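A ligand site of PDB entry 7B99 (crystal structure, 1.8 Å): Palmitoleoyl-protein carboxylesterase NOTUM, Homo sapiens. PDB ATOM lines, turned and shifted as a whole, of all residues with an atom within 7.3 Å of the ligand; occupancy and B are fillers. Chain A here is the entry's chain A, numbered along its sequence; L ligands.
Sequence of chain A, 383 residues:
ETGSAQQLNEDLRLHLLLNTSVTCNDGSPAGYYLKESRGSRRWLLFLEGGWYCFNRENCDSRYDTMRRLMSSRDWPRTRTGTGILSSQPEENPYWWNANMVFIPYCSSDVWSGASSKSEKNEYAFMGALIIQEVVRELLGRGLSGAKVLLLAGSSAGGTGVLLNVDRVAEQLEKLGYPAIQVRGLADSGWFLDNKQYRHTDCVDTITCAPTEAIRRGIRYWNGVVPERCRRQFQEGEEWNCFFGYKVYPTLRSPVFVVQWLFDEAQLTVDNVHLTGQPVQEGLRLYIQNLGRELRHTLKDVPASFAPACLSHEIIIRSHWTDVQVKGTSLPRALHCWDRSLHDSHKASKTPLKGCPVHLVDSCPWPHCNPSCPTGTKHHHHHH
OD1 of Asn 194 lies close to O of Leu 192 (3.4 Å).
The side-chain amide oxygen (OD1) of Asn 194 lies within hydrogen-bond range of the side-chain amide nitrogen (NE2) of Gln 266 (3.3 Å).
OD1 of Asn 194 lies close to OD1 of Asp 270 (2.8 Å).
O of Val 269 sits at hydrogen-bond distance from NE2 of Gln 196, at 2.9 Å.
The backbone NH (N) of Leu 192 sits at hydrogen-bond distance from the side-chain amide oxygen (OE1) of Gln 266.
The side-chain amide nitrogen (NE2) of Gln 266 sits at hydrogen-bond distance from the side-chain carboxylate (OD2) of Asp 270 (3.1 Å).
OD2 of Asp 263 is in hydrogen-bond range of N of Gln 266 (3.0 Å).
The backbone carbonyl oxygen of Asn 194 is in hydrogen-bond range of a nitrogen (N1) of the ligand (2.4 Å).
The backbone carbonyl oxygen (O) of Asp 193 lies close to a nitrogen (N1) of the ligand (3.5 Å).
Phe 191 touches the ligand (CB to C7, 3.4 Å).
Leu 192 touches the ligand.
CG2 of Thr 211 touches C1 of the ligand, 3.3 Å away.
Phe 243 touches the ligand (CZ to C2, 3.7 Å).
OE1 of Gln 266 touches C7 of the ligand, at 3.8 Å.
CG2 of Val 269 touches C12 of the ligand (3.6 Å).
Hydrophobic or aromatic side chains within 4 Å of the ligand: Phe 191, Phe 243 and Val 269.
Eight residues have an atom within 4 Å of the ligand: Phe 191, Leu 192, Asp 193, Asn 194, Thr 211, Phe 243, Gln 266 and Val 269.
Along chain A the residues within 4 Å of the ligand span positions 191 to 269.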
ATOM      1  N   TRP A  51     -13.479  11.093 -24.280  1.00  0.00           N
ATOM      2  CA  TRP A  51     -13.156  10.967 -22.853  1.00  0.00           C
ATOM      3  C   TRP A  51     -11.886  11.754 -22.501  1.00  0.00           C
ATOM      4  O   TRP A  51     -11.706  12.863 -23.009  1.00  0.00           O
ATOM      5  CB  TRP A  51     -13.057   9.500 -22.442  1.00  0.00           C
ATOM      6  CG  TRP A  51     -14.397   8.765 -22.539  1.00  0.00           C
ATOM      7  CD1 TRP A  51     -14.810   7.926 -23.547  1.00  0.00           C
ATOM      8  CD2 TRP A  51     -15.518   8.859 -21.630  1.00  0.00           C
ATOM      9  NE1 TRP A  51     -16.085   7.474 -23.298  1.00  0.00           N
ATOM     10  CE2 TRP A  51     -16.547   8.035 -22.140  1.00  0.00           C
ATOM     11  CE3 TRP A  51     -15.741   9.547 -20.433  1.00  0.00           C
ATOM     12  CZ2 TRP A  51     -17.768   7.881 -21.490  1.00  0.00           C
ATOM     13  CZ3 TRP A  51     -16.959   9.397 -19.799  1.00  0.00           C
ATOM     14  CH2 TRP A  51     -17.961   8.566 -20.326  1.00  0.00           C
ATOM     15  N   TYR A  52     -11.027  11.216 -21.623  1.00  0.00           N
ATOM     16  CA  TYR A  52      -9.842  11.935 -21.113  1.00  0.00           C
ATOM     17  C   TYR A  52      -9.061  10.994 -20.192  1.00  0.00           C
ATOM     18  O   TYR A  52      -9.511   9.901 -19.868  1.00  0.00           O
ATOM     19  CB  TYR A  52     -10.254  13.225 -20.397  1.00  0.00           C
ATOM     20  CG  TYR A  52     -11.125  13.051 -19.162  1.00  0.00           C
ATOM     21  CD1 TYR A  52     -12.485  13.341 -19.207  1.00  0.00           C
ATOM     22  CD2 TYR A  52     -10.576  12.696 -17.933  1.00  0.00           C
ATOM     23  CE1 TYR A  52     -13.294  13.200 -18.083  1.00  0.00           C
ATOM     24  CE2 TYR A  52     -11.376  12.577 -16.802  1.00  0.00           C
ATOM     25  CZ  TYR A  52     -12.737  12.825 -16.893  1.00  0.00           C
ATOM     26  OH  TYR A  52     -13.530  12.703 -15.774  1.00  0.00           O
ATOM     27  N   TRP A 190     -23.392  18.244 -21.783  1.00  0.00           N
ATOM     28  CA  TRP A 190     -24.190  18.855 -20.712  1.00  0.00           C
ATOM     29  C   TRP A 190     -24.532  17.755 -19.703  1.00  0.00           C
ATOM     30  O   TRP A 190     -25.548  17.067 -19.841  1.00  0.00           O
ATOM     31  CB  TRP A 190     -25.456  19.479 -21.303  1.00  0.00           C
ATOM     32  CG  TRP A 190     -26.329  20.275 -20.372  1.00  0.00           C
ATOM     33  CD1 TRP A 190     -27.327  19.791 -19.573  1.00  0.00           C
ATOM     34  CD2 TRP A 190     -26.352  21.704 -20.222  1.00  0.00           C
ATOM     35  NE1 TRP A 190     -27.932  20.823 -18.897  1.00  0.00           N
ATOM     36  CE2 TRP A 190     -27.356  21.999 -19.272  1.00  0.00           C
ATOM     37  CE3 TRP A 190     -25.595  22.746 -20.767  1.00  0.00           C
ATOM     38  CZ2 TRP A 190     -27.625  23.320 -18.872  1.00  0.00           C
ATOM     39  CZ3 TRP A 190     -25.882  24.043 -20.369  1.00  0.00           C
ATOM     40  CH2 TRP A 190     -26.886  24.318 -19.429  1.00  0.00           C
ATOM     41  N   PHE A 191     -23.699  17.604 -18.669  1.00  0.00           N
ATOM     42  CA  PHE A 191     -23.820  16.480 -17.758  1.00  0.00           C
ATOM     43  C   PHE A 191     -24.252  16.922 -16.356  1.00  0.00           C
ATOM     44  O   PHE A 191     -24.146  18.095 -15.999  1.00  0.00           O
ATOM     45  CB  PHE A 191     -22.503  15.700 -17.674  1.00  0.00           C
ATOM     46  CG  PHE A 191     -22.030  15.175 -18.996  1.00  0.00           C
ATOM     47  CD1 PHE A 191     -20.997  15.794 -19.676  1.00  0.00           C
ATOM     48  CD2 PHE A 191     -22.670  14.098 -19.601  1.00  0.00           C
ATOM     49  CE1 PHE A 191     -20.562  15.331 -20.904  1.00  0.00           C
ATOM     50  CE2 PHE A 191     -22.246  13.626 -20.833  1.00  0.00           C
ATOM     51  CZ  PHE A 191     -21.199  14.243 -21.488  1.00  0.00           C
ATOM     52  N   LEU A 192     -24.736  15.949 -15.579  1.00  0.00           N
ATOM     53  CA  LEU A 192     -25.248  16.186 -14.238  1.00  0.00           C
ATOM     54  C   LEU A 192     -24.371  15.454 -13.223  1.00  0.00           C
ATOM     55  O   LEU A 192     -24.005  14.293 -13.438  1.00  0.00           O
ATOM     56  CB  LEU A 192     -26.692  15.684 -14.098  1.00  0.00           C
ATOM     57  CG  LEU A 192     -27.770  16.301 -15.002  1.00  0.00           C
ATOM     58  CD1 LEU A 192     -29.121  15.639 -14.720  1.00  0.00           C
ATOM     59  CD2 LEU A 192     -27.854  17.805 -14.842  1.00  0.00           C
ATOM     60  N   ASP A 193     -24.037  16.138 -12.135  1.00  0.00           N
ATOM     61  CA  ASP A 193     -23.315  15.502 -11.033  1.00  0.00           C
ATOM     62  C   ASP A 193     -24.334  14.940 -10.022  1.00  0.00           C
ATOM     63  O   ASP A 193     -24.435  15.374  -8.881  1.00  0.00           O
ATOM     64  CB  ASP A 193     -22.348  16.484 -10.381  1.00  0.00           C
ATOM     65  CG  ASP A 193     -22.981  17.825 -10.049  1.00  0.00           C
ATOM     66  OD1 ASP A 193     -24.068  18.138 -10.587  1.00  0.00           O
ATOM     67  OD2 ASP A 193     -22.389  18.584  -9.253  1.00  0.00           O
ATOM     68  N   ASN A 194     -25.080  13.933 -10.482  1.00  0.00           N
ATOM     69  CA  ASN A 194     -26.220  13.411  -9.756  1.00  0.00           C
ATOM     70  C   ASN A 194     -25.836  12.190  -8.928  1.00  0.00           C
ATOM     71  O   ASN A 194     -24.705  11.703  -8.960  1.00  0.00           O
ATOM     72  CB  ASN A 194     -27.367  13.066 -10.696  1.00  0.00           C
ATOM     73  CG  ASN A 194     -26.974  12.049 -11.757  1.00  0.00           C
ATOM     74  OD1 ASN A 194     -25.793  11.751 -11.955  1.00  0.00           O
ATOM     75  ND2 ASN A 194     -27.972  11.483 -12.432  1.00  0.00           N
ATOM     76  N   LYS A 195     -26.817  11.668  -8.184  1.00  0.00           N
ATOM     77  CA  LYS A 195     -26.629  10.428  -7.455  1.00  0.00           C
ATOM     78  C   LYS A 195     -26.607   9.251  -8.423  1.00  0.00           C
ATOM     79  O   LYS A 195     -27.456   9.141  -9.310  1.00  0.00           O
ATOM     80  CB  LYS A 195     -27.751  10.241  -6.425  1.00  0.00           C
ATOM     81  N   GLN A 196     -25.610   8.380  -8.266  1.00  0.00           N
ATOM     82  CA  GLN A 196     -25.490   7.207  -9.108  1.00  0.00           C
ATOM     83  C   GLN A 196     -26.563   6.177  -8.771  1.00  0.00           C
ATOM     84  O   GLN A 196     -27.091   6.129  -7.658  1.00  0.00           O
ATOM     85  CB  GLN A 196     -24.106   6.565  -8.932  1.00  0.00           C
ATOM     86  CG  GLN A 196     -22.985   7.248  -9.676  1.00  0.00           C
ATOM     87  CD  GLN A 196     -21.634   6.711  -9.259  1.00  0.00           C
ATOM     88  OE1 GLN A 196     -21.433   6.357  -8.100  1.00  0.00           O
ATOM     89  NE2 GLN A 196     -20.719   6.614 -10.210  1.00  0.00           N
ATOM     90  N   THR A 211     -16.600  12.341  -9.118  1.00  0.00           N
ATOM     91  CA  THR A 211     -16.028  13.677  -9.212  1.00  0.00           C
ATOM     92  C   THR A 211     -14.537  13.691  -8.975  1.00  0.00           C
ATOM     93  O   THR A 211     -13.872  14.675  -9.275  1.00  0.00           O
ATOM     94  CB  THR A 211     -16.651  14.650  -8.194  1.00  0.00           C
ATOM     95  OG1 THR A 211     -16.444  14.167  -6.867  1.00  0.00           O
ATOM     96  CG2 THR A 211     -18.121  14.840  -8.442  1.00  0.00           C
ATOM     97  N   GLU A 212     -13.999  12.614  -8.400  1.00  0.00           N
ATOM     98  CA  GLU A 212     -12.590  12.636  -8.093  1.00  0.00           C
ATOM     99  C   GLU A 212     -11.748  12.600  -9.362  1.00  0.00           C
ATOM    100  O   GLU A 212     -10.702  13.220  -9.402  1.00  0.00           O
ATOM    101  CB  GLU A 212     -12.204  11.488  -7.153  1.00  0.00           C
ATOM    102  CG  GLU A 212     -10.907  11.758  -6.368  1.00  0.00           C
ATOM    103  CD  GLU A 212     -10.930  13.057  -5.563  1.00  0.00           C
ATOM    104  OE1 GLU A 212     -12.017  13.649  -5.365  1.00  0.00           O
ATOM    105  OE2 GLU A 212      -9.846  13.497  -5.127  1.00  0.00           O
ATOM    106  N   ILE A 214     -12.305  14.091 -12.222  1.00  0.00           N
ATOM    107  CA  ILE A 214     -12.145  15.431 -12.805  1.00  0.00           C
ATOM    108  C   ILE A 214     -11.383  16.377 -11.893  1.00  0.00           C
ATOM    109  O   ILE A 214     -10.666  17.267 -12.370  1.00  0.00           O
ATOM    110  CB  ILE A 214     -13.512  16.026 -13.199  1.00  0.00           C
ATOM    111  CG1 ILE A 214     -13.332  17.303 -14.026  1.00  0.00           C
ATOM    112  CG2 ILE A 214     -14.388  16.278 -11.975  1.00  0.00           C
ATOM    113  CD1 ILE A 214     -12.448  17.111 -15.247  1.00  0.00           C
ATOM    114  N   TRP A 239     -13.587  22.406 -10.655  1.00  0.00           N
ATOM    115  CA  TRP A 239     -14.242  21.269 -11.301  1.00  0.00           C
ATOM    116  C   TRP A 239     -15.716  21.526 -11.563  1.00  0.00           C
ATOM    117  O   TRP A 239     -16.294  20.967 -12.497  1.00  0.00           O
ATOM    118  CB  TRP A 239     -14.092  19.999 -10.457  1.00  0.00           C
ATOM    119  CG  TRP A 239     -14.858  19.996  -9.153  1.00  0.00           C
ATOM    120  CD1 TRP A 239     -14.376  20.317  -7.921  1.00  0.00           C
ATOM    121  CD2 TRP A 239     -16.253  19.661  -8.963  1.00  0.00           C
ATOM    122  NE1 TRP A 239     -15.366  20.206  -6.978  1.00  0.00           N
ATOM    123  CE2 TRP A 239     -16.522  19.804  -7.580  1.00  0.00           C
ATOM    124  CE3 TRP A 239     -17.280  19.258  -9.813  1.00  0.00           C
ATOM    125  CZ2 TRP A 239     -17.784  19.556  -7.039  1.00  0.00           C
ATOM    126  CZ3 TRP A 239     -18.534  19.013  -9.276  1.00  0.00           C
ATOM    127  CH2 TRP A 239     -18.777  19.163  -7.906  1.00  0.00           C
ATOM    128  N   PHE A 243     -19.480  21.388 -15.468  1.00  0.00           N
ATOM    129  CA  PHE A 243     -20.872  20.965 -15.524  1.00  0.00           C
ATOM    130  C   PHE A 243     -21.723  22.079 -16.103  1.00  0.00           C
ATOM    131  O   PHE A 243     -21.816  23.166 -15.528  1.00  0.00           O
ATOM    132  CB  PHE A 243     -21.368  20.517 -14.152  1.00  0.00           C
ATOM    133  CG  PHE A 243     -20.757  19.230 -13.706  1.00  0.00           C
ATOM    134  CD1 PHE A 243     -19.464  19.187 -13.207  1.00  0.00           C
ATOM    135  CD2 PHE A 243     -21.440  18.037 -13.890  1.00  0.00           C
ATOM    136  CE1 PHE A 243     -18.887  17.981 -12.829  1.00  0.00           C
ATOM    137  CE2 PHE A 243     -20.870  16.833 -13.525  1.00  0.00           C
ATOM    138  CZ  PHE A 243     -19.587  16.803 -12.994  1.00  0.00           C
ATOM    139  N   ASP A 263     -28.814  10.407 -21.999  1.00  0.00           N
ATOM    140  CA  ASP A 263     -27.522  10.319 -22.661  1.00  0.00           C
ATOM    141  C   ASP A 263     -26.752   9.090 -22.189  1.00  0.00           C
ATOM    142  O   ASP A 263     -26.699   8.785 -21.000  1.00  0.00           O
ATOM    143  CB  ASP A 263     -26.719  11.593 -22.379  1.00  0.00           C
ATOM    144  CG  ASP A 263     -25.376  11.596 -23.049  1.00  0.00           C
ATOM    145  OD1 ASP A 263     -25.296  12.042 -24.220  1.00  0.00           O
ATOM    146  OD2 ASP A 263     -24.396  11.152 -22.427  1.00  0.00           O
ATOM    147  N   ALA A 265     -23.493   8.385 -22.194  1.00  0.00           N
ATOM    148  CA  ALA A 265     -22.338   8.649 -21.349  1.00  0.00           C
ATOM    149  C   ALA A 265     -22.769   8.961 -19.922  1.00  0.00           C
ATOM    150  O   ALA A 265     -22.152   8.490 -18.962  1.00  0.00           O
ATOM    151  CB  ALA A 265     -21.502   9.793 -21.933  1.00  0.00           C
ATOM    152  N   GLN A 266     -23.834   9.757 -19.777  1.00  0.00           N
ATOM    153  CA  GLN A 266     -24.402  10.026 -18.459  1.00  0.00           C
ATOM    154  C   GLN A 266     -24.812   8.736 -17.751  1.00  0.00           C
ATOM    155  O   GLN A 266     -24.507   8.548 -16.572  1.00  0.00           O
ATOM    156  CB  GLN A 266     -25.620  10.954 -18.611  1.00  0.00           C
ATOM    157  CG  GLN A 266     -26.324  11.320 -17.305  1.00  0.00           C
ATOM    158  CD  GLN A 266     -25.565  12.330 -16.457  1.00  0.00           C
ATOM    159  OE1 GLN A 266     -25.153  13.391 -16.942  1.00  0.00           O
ATOM    160  NE2 GLN A 266     -25.382  12.013 -15.178  1.00  0.00           N
ATOM    161  N   LEU A 267     -25.498   7.842 -18.464  1.00  0.00           N
ATOM    162  CA  LEU A 267     -25.966   6.613 -17.815  1.00  0.00           C
ATOM    163  C   LEU A 267     -24.809   5.676 -17.493  1.00  0.00           C
ATOM    164  O   LEU A 267     -24.891   4.924 -16.511  1.00  0.00           O
ATOM    165  CB  LEU A 267     -27.009   5.920 -18.690  1.00  0.00           C
ATOM    166  CG  LEU A 267     -28.377   6.592 -18.751  1.00  0.00           C
ATOM    167  CD1 LEU A 267     -29.203   5.990 -19.855  1.00  0.00           C
ATOM    168  CD2 LEU A 267     -29.109   6.466 -17.423  1.00  0.00           C
ATOM    169  N   THR A 268     -23.747   5.690 -18.301  1.00  0.00           N
ATOM    170  CA  THR A 268     -22.580   4.873 -17.987  1.00  0.00           C
ATOM    171  C   THR A 268     -21.949   5.287 -16.663  1.00  0.00           C
ATOM    172  O   THR A 268     -21.734   4.451 -15.779  1.00  0.00           O
ATOM    173  CB  THR A 268     -21.555   4.964 -19.122  1.00  0.00           C
ATOM    174  OG1 THR A 268     -22.048   4.298 -20.284  1.00  0.00           O
ATOM    175  CG2 THR A 268     -20.229   4.326 -18.694  1.00  0.00           C
ATOM    176  N   VAL A 269     -21.667   6.582 -16.508  1.00  0.00           N
ATOM    177  CA  VAL A 269     -21.074   7.066 -15.268  1.00  0.00           C
ATOM    178  C   VAL A 269     -22.021   6.848 -14.094  1.00  0.00           C
ATOM    179  O   VAL A 269     -21.575   6.669 -12.950  1.00  0.00           O
ATOM    180  CB  VAL A 269     -20.670   8.549 -15.432  1.00  0.00           C
ATOM    181  CG1 VAL A 269     -20.112   9.103 -14.133  1.00  0.00           C
ATOM    182  CG2 VAL A 269     -19.650   8.687 -16.551  1.00  0.00           C
ATOM    183  N   ASP A 270     -23.331   6.830 -14.341  1.00  0.00           N
ATOM    184  CA  ASP A 270     -24.319   6.539 -13.306  1.00  0.00           C
ATOM    185  C   ASP A 270     -24.461   5.053 -12.993  1.00  0.00           C
ATOM    186  O   ASP A 270     -25.263   4.704 -12.124  1.00  0.00           O
ATOM    187  CB  ASP A 270     -25.683   7.104 -13.689  1.00  0.00           C
ATOM    188  CG  ASP A 270     -25.769   8.604 -13.513  1.00  0.00           C
ATOM    189  OD1 ASP A 270     -25.101   9.138 -12.599  1.00  0.00           O
ATOM    190  OD2 ASP A 270     -26.524   9.257 -14.264  1.00  0.00           O
ATOM    191  N   TYR A 286     -35.540   5.820 -11.398  1.00  0.00           N
ATOM    192  CA  TYR A 286     -34.244   6.460 -11.620  1.00  0.00           C
ATOM    193  C   TYR A 286     -34.162   7.091 -13.004  1.00  0.00           C
ATOM    194  O   TYR A 286     -33.767   8.248 -13.154  1.00  0.00           O
ATOM    195  CB  TYR A 286     -33.100   5.466 -11.420  1.00  0.00           C
ATOM    196  CG  TYR A 286     -31.733   6.126 -11.467  1.00  0.00           C
ATOM    197  CD1 TYR A 286     -31.127   6.598 -10.300  1.00  0.00           C
ATOM    198  CD2 TYR A 286     -31.073   6.325 -12.674  1.00  0.00           C
ATOM    199  CE1 TYR A 286     -29.897   7.219 -10.342  1.00  0.00           C
ATOM    200  CE2 TYR A 286     -29.835   6.949 -12.721  1.00  0.00           C
ATOM    201  CZ  TYR A 286     -29.260   7.401 -11.555  1.00  0.00           C
ATOM    202  OH  TYR A 286     -28.030   8.023 -11.598  1.00  0.00           O
HETATM  203  N1  LIG L   1     -22.463  12.532  -8.742  1.00  0.00           N
HETATM  204  C1  LIG L   1     -20.600  13.454 -10.078  1.00  0.00           C
HETATM  205  C2  LIG L   1     -19.876  13.548 -11.259  1.00  0.00           C
HETATM  206  C3  LIG L   1     -20.247  12.826 -12.373  1.00  0.00           C
HETATM  207  C4  LIG L   1     -21.355  11.980 -12.277  1.00  0.00           C
HETATM  208  C5  LIG L   1     -22.070  11.888 -11.101  1.00  0.00           C
HETATM  209  C6  LIG L   1     -18.850  12.410 -15.879  1.00  0.00           C
HETATM  210  C7  LIG L   1     -21.473  12.553 -16.714  1.00  0.00           C
HETATM  211  C8  LIG L   1     -22.971  12.782  -6.230  1.00  0.00           C
HETATM  212  C9  LIG L   1     -22.026  12.973  -7.422  1.00  0.00           C
HETATM  213  O1  LIG L   1     -20.963  13.460  -7.229  1.00  0.00           O
HETATM  214  C10 LIG L   1     -21.701  12.624  -9.985  1.00  0.00           C
HETATM  215  N2  LIG L   1     -19.435  12.970 -13.580  1.00  0.00           N
HETATM  216  C11 LIG L   1     -19.839  12.721 -14.959  1.00  0.00           C
HETATM  217  C12 LIG L   1     -19.162  12.167 -17.210  1.00  0.00           C
HETATM  218  C13 LIG L   1     -20.481  12.248 -17.626  1.00  0.00           C
HETATM  219  C14 LIG L   1     -21.152  12.799 -15.387  1.00  0.00           C
